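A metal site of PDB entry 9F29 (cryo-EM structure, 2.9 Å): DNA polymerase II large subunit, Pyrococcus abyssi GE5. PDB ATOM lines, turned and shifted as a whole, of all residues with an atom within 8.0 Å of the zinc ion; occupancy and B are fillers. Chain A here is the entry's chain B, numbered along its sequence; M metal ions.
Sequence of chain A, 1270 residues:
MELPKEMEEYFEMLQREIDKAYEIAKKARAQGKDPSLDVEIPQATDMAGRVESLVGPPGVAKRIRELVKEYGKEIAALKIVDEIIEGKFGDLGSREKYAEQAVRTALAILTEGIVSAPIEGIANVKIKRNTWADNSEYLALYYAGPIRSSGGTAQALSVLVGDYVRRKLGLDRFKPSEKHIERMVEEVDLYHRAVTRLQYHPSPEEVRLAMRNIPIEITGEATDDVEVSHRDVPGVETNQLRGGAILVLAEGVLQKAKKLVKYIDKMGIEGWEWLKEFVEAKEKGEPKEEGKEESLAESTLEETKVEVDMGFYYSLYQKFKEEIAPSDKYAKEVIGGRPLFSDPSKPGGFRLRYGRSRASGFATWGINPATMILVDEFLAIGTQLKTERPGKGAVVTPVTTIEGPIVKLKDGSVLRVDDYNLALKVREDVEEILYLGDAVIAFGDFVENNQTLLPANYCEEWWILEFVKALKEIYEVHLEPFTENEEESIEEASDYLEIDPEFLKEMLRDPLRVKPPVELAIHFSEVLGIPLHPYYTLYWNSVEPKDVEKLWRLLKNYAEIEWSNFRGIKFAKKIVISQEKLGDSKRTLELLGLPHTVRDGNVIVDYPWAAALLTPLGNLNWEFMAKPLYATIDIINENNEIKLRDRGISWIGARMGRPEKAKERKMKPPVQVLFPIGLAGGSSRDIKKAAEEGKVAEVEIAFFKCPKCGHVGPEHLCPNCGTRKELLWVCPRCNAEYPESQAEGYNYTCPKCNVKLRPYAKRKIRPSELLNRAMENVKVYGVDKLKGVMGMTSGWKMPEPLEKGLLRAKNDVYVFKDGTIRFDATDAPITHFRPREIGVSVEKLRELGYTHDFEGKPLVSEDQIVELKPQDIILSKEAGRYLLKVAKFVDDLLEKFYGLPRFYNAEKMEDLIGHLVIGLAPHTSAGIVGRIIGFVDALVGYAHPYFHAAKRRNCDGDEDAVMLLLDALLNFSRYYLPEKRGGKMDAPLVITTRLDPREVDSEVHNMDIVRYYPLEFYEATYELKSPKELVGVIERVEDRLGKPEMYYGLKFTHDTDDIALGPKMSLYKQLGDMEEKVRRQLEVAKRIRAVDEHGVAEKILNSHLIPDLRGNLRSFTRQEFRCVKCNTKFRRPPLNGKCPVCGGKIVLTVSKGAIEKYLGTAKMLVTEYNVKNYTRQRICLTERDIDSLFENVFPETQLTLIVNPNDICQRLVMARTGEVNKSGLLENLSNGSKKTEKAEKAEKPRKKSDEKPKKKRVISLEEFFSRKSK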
ATOM      1  N   LYS A 705     -31.119  -8.836   1.057  1.00  0.00           N
ATOM      2  CA  LYS A 705     -29.726  -8.705   0.639  1.00  0.00           C
ATOM      3  C   LYS A 705     -29.338  -7.234   0.570  1.00  0.00           C
ATOM      4  O   LYS A 705     -30.062  -6.426  -0.024  1.00  0.00           O
ATOM      5  CB  LYS A 705     -29.481  -9.368  -0.705  1.00  0.00           C
ATOM      6  CG  LYS A 705     -28.019  -9.491  -1.083  1.00  0.00           C
ATOM      7  CD  LYS A 705     -27.842 -10.315  -2.341  1.00  0.00           C
ATOM      8  CE  LYS A 705     -26.375 -10.536  -2.648  1.00  0.00           C
ATOM      9  NZ  LYS A 705     -25.723 -11.380  -1.597  1.00  0.00           N
ATOM     10  N   CYS A 706     -28.191  -6.894   1.146  1.00  0.00           N
ATOM     11  CA  CYS A 706     -27.700  -5.519   1.145  1.00  0.00           C
ATOM     12  C   CYS A 706     -27.063  -5.195  -0.200  1.00  0.00           C
ATOM     13  O   CYS A 706     -26.237  -5.968  -0.689  1.00  0.00           O
ATOM     14  CB  CYS A 706     -26.698  -5.305   2.276  1.00  0.00           C
ATOM     15  SG  CYS A 706     -26.088  -3.610   2.443  1.00  0.00           S
ATOM     16  N   PRO A 707     -27.425  -4.074  -0.827  1.00  0.00           N
ATOM     17  CA  PRO A 707     -26.847  -3.755  -2.147  1.00  0.00           C
ATOM     18  C   PRO A 707     -25.344  -3.569  -2.129  1.00  0.00           C
ATOM     19  O   PRO A 707     -24.680  -3.897  -3.126  1.00  0.00           O
ATOM     20  CB  PRO A 707     -27.567  -2.460  -2.530  1.00  0.00           C
ATOM     21  CG  PRO A 707     -28.783  -2.406  -1.662  1.00  0.00           C
ATOM     22  CD  PRO A 707     -28.402  -3.072  -0.388  1.00  0.00           C
ATOM     23  N   LYS A 708     -24.771  -3.049  -1.042  1.00  0.00           N
ATOM     24  CA  LYS A 708     -23.358  -2.696  -1.023  1.00  0.00           C
ATOM     25  C   LYS A 708     -22.482  -3.809  -0.448  1.00  0.00           C
ATOM     26  O   LYS A 708     -21.575  -4.296  -1.126  1.00  0.00           O
ATOM     27  CB  LYS A 708     -23.172  -1.402  -0.223  1.00  0.00           C
ATOM     28  CG  LYS A 708     -23.544  -0.144  -0.984  1.00  0.00           C
ATOM     29  CD  LYS A 708     -23.305   1.098  -0.139  1.00  0.00           C
ATOM     30  CE  LYS A 708     -24.385   1.264   0.914  1.00  0.00           C
ATOM     31  NZ  LYS A 708     -25.725   1.456   0.296  1.00  0.00           N
ATOM     32  N   CYS A 709     -22.732  -4.201   0.801  1.00  0.00           N
ATOM     33  CA  CYS A 709     -21.854  -5.127   1.487  1.00  0.00           C
ATOM     34  C   CYS A 709     -22.169  -6.591   1.227  1.00  0.00           C
ATOM     35  O   CYS A 709     -21.306  -7.452   1.443  1.00  0.00           O
ATOM     36  CB  CYS A 709     -21.889  -4.873   2.993  1.00  0.00           C
ATOM     37  SG  CYS A 709     -23.247  -5.684   3.857  1.00  0.00           S
ATOM     38  N   GLY A 710     -23.386  -6.914   0.767  1.00  0.00           N
ATOM     39  CA  GLY A 710     -23.722  -8.285   0.469  1.00  0.00           C
ATOM     40  C   GLY A 710     -24.204  -9.110   1.645  1.00  0.00           C
ATOM     41  O   GLY A 710     -24.133 -10.346   1.579  1.00  0.00           O
ATOM     42  N   HIS A 711     -24.695  -8.487   2.703  1.00  0.00           N
ATOM     43  CA  HIS A 711     -25.206  -9.223   3.846  1.00  0.00           C
ATOM     44  C   HIS A 711     -26.540  -9.881   3.511  1.00  0.00           C
ATOM     45  O   HIS A 711     -27.338  -9.333   2.750  1.00  0.00           O
ATOM     46  CB  HIS A 711     -25.355  -8.295   5.049  1.00  0.00           C
ATOM     47  CG  HIS A 711     -25.654  -9.013   6.332  1.00  0.00           C
ATOM     48  ND1 HIS A 711     -24.896 -10.062   6.786  1.00  0.00           N
ATOM     49  CD2 HIS A 711     -26.616  -8.813   7.268  1.00  0.00           C
ATOM     50  CE1 HIS A 711     -25.373 -10.491   7.937  1.00  0.00           C
ATOM     51  NE2 HIS A 711     -26.422  -9.752   8.255  1.00  0.00           N
ATOM     52  N   VAL A 712     -26.775 -11.052   4.095  1.00  0.00           N
ATOM     53  CA  VAL A 712     -28.021 -11.799   3.897  1.00  0.00           C
ATOM     54  C   VAL A 712     -28.593 -12.143   5.270  1.00  0.00           C
ATOM     55  O   VAL A 712     -27.885 -12.684   6.125  1.00  0.00           O
ATOM     56  CB  VAL A 712     -27.801 -13.074   3.068  1.00  0.00           C
ATOM     57  CG1 VAL A 712     -29.088 -13.844   2.931  1.00  0.00           C
ATOM     58  CG2 VAL A 712     -27.240 -12.725   1.702  1.00  0.00           C
ATOM     59  N   LEU A 717     -32.981  -3.746   7.888  1.00  0.00           N
ATOM     60  CA  LEU A 717     -31.866  -2.810   7.902  1.00  0.00           C
ATOM     61  C   LEU A 717     -30.556  -3.567   8.106  1.00  0.00           C
ATOM     62  O   LEU A 717     -30.489  -4.501   8.901  1.00  0.00           O
ATOM     63  CB  LEU A 717     -32.045  -1.758   8.993  1.00  0.00           C
ATOM     64  CG  LEU A 717     -32.739  -0.459   8.593  1.00  0.00           C
ATOM     65  CD1 LEU A 717     -32.662   0.546   9.731  1.00  0.00           C
ATOM     66  CD2 LEU A 717     -32.140   0.124   7.332  1.00  0.00           C
ATOM     67  N   CYS A 718     -29.528  -3.149   7.389  1.00  0.00           N
ATOM     68  CA  CYS A 718     -28.236  -3.830   7.434  1.00  0.00           C
ATOM     69  C   CYS A 718     -27.556  -3.572   8.773  1.00  0.00           C
ATOM     70  O   CYS A 718     -27.336  -2.416   9.135  1.00  0.00           O
ATOM     71  CB  CYS A 718     -27.363  -3.352   6.287  1.00  0.00           C
ATOM     72  SG  CYS A 718     -25.719  -4.096   6.222  1.00  0.00           S
ATOM     73  N   PRO A 719     -27.208  -4.618   9.534  1.00  0.00           N
ATOM     74  CA  PRO A 719     -26.539  -4.385  10.831  1.00  0.00           C
ATOM     75  C   PRO A 719     -25.176  -3.742  10.719  1.00  0.00           C
ATOM     76  O   PRO A 719     -24.706  -3.147  11.700  1.00  0.00           O
ATOM     77  CB  PRO A 719     -26.458  -5.786  11.442  1.00  0.00           C
ATOM     78  CG  PRO A 719     -26.707  -6.735  10.322  1.00  0.00           C
ATOM     79  CD  PRO A 719     -27.558  -6.033   9.325  1.00  0.00           C
ATOM     80  N   ASN A 720     -24.507  -3.834   9.575  1.00  0.00           N
ATOM     81  CA  ASN A 720     -23.187  -3.239   9.390  1.00  0.00           C
ATOM     82  C   ASN A 720     -23.255  -1.913   8.645  1.00  0.00           C
ATOM     83  O   ASN A 720     -22.794  -0.884   9.152  1.00  0.00           O
ATOM     84  CB  ASN A 720     -22.270  -4.222   8.647  1.00  0.00           C
ATOM     85  CG  ASN A 720     -22.150  -5.549   9.348  1.00  0.00           C
ATOM     86  OD1 ASN A 720     -22.036  -5.619  10.574  1.00  0.00           O
ATOM     87  ND2 ASN A 720     -22.178  -6.630   8.575  1.00  0.00           N
ATOM     88  N   CYS A 721     -23.837  -1.915   7.446  1.00  0.00           N
ATOM     89  CA  CYS A 721     -23.918  -0.689   6.653  1.00  0.00           C
ATOM     90  C   CYS A 721     -24.914   0.288   7.256  1.00  0.00           C
ATOM     91  O   CYS A 721     -24.614   1.480   7.416  1.00  0.00           O
ATOM     92  CB  CYS A 721     -24.307  -1.024   5.218  1.00  0.00           C
ATOM     93  SG  CYS A 721     -23.109  -2.000   4.308  1.00  0.00           S
ATOM     94  N   GLY A 722     -26.099  -0.204   7.614  1.00  0.00           N
ATOM     95  CA  GLY A 722     -27.186   0.654   8.038  1.00  0.00           C
ATOM     96  C   GLY A 722     -28.185   1.004   6.946  1.00  0.00           C
ATOM     97  O   GLY A 722     -29.119   1.764   7.216  1.00  0.00           O
ATOM     98  N   THR A 723     -28.023   0.465   5.748  1.00  0.00           N
ATOM     99  CA  THR A 723     -28.891   0.780   4.630  1.00  0.00           C
ATOM    100  C   THR A 723     -30.005  -0.263   4.499  1.00  0.00           C
ATOM    101  O   THR A 723     -29.978  -1.325   5.129  1.00  0.00           O
ATOM    102  CB  THR A 723     -28.108   0.845   3.322  1.00  0.00           C
ATOM    103  OG1 THR A 723     -27.386  -0.390   3.129  1.00  0.00           O
ATOM    104  CG2 THR A 723     -27.108   1.985   3.368  1.00  0.00           C
ATOM    105  N   ARG A 724     -30.999   0.059   3.674  1.00  0.00           N
ATOM    106  CA  ARG A 724     -32.128  -0.830   3.460  1.00  0.00           C
ATOM    107  C   ARG A 724     -31.768  -1.913   2.455  1.00  0.00           C
ATOM    108  O   ARG A 724     -31.116  -1.642   1.439  1.00  0.00           O
ATOM    109  CB  ARG A 724     -33.343  -0.043   2.986  1.00  0.00           C
ATOM    110  CG  ARG A 724     -34.659  -0.701   3.340  1.00  0.00           C
ATOM    111  CD  ARG A 724     -35.833   0.179   3.001  1.00  0.00           C
ATOM    112  NE  ARG A 724     -36.986  -0.605   2.600  1.00  0.00           N
ATOM    113  CZ  ARG A 724     -37.878  -1.115   3.447  1.00  0.00           C
ATOM    114  NH1 ARG A 724     -37.761  -0.934   4.755  1.00  0.00           N
ATOM    115  NH2 ARG A 724     -38.892  -1.829   2.976  1.00  0.00           N
ATOM    116  N   LYS A 725     -32.213  -3.125   2.727  1.00  0.00           N
ATOM    117  CA  LYS A 725     -31.910  -4.285   1.904  1.00  0.00           C
ATOM    118  C   LYS A 725     -33.080  -4.610   0.975  1.00  0.00           C
ATOM    119  O   LYS A 725     -34.184  -4.078   1.117  1.00  0.00           O
ATOM    120  CB  LYS A 725     -31.563  -5.490   2.781  1.00  0.00           C
ATOM    121  CG  LYS A 725     -30.488  -5.208   3.814  1.00  0.00           C
ATOM    122  CD  LYS A 725     -29.786  -6.474   4.259  1.00  0.00           C
ATOM    123  CE  LYS A 725     -30.468  -7.097   5.450  1.00  0.00           C
ATOM    124  NZ  LYS A 725     -29.806  -8.359   5.873  1.00  0.00           N
HETATM  125 ZN    ZN M   1     -24.583  -3.809   4.214  1.00  0.00          ZN
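N of Cys 718 is in hydrogen-bond range of O of Thr 723, at 2.9 Å.
SG of Cys 718 sits close to N of Asn 720.
SG of Cys 709 sits close to N of His 711 (3.4 Å).
The side-chain sulfur (SG) of Cys 706 sits close to the side-chain hydroxyl (OG1) of Thr 723 (3.5 Å).
The backbone NH (N) of Cys 706 is in hydrogen-bond range of the backbone carbonyl oxygen (O) of His 711, 3.0 Å away.
The backbone NH (N) of Lys 708 sits close to the side-chain sulfur (SG) of Cys 706 (3.8 Å).
Of the 17 residues printed, 4 come within 4 Å of the zinc ion.
The zinc ion is bound by the side-chain sulfur (SG) of Cys 718 (2.3 Å), the side-chain sulfur (SG) of Cys 709 (2.3 Å), the side-chain sulfur (SG) of Cys 706 (2.3 Å) and the side-chain sulfur (SG) of Cys 721 (2.3 Å).
The zinc ion has four donor atoms within binding distance.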
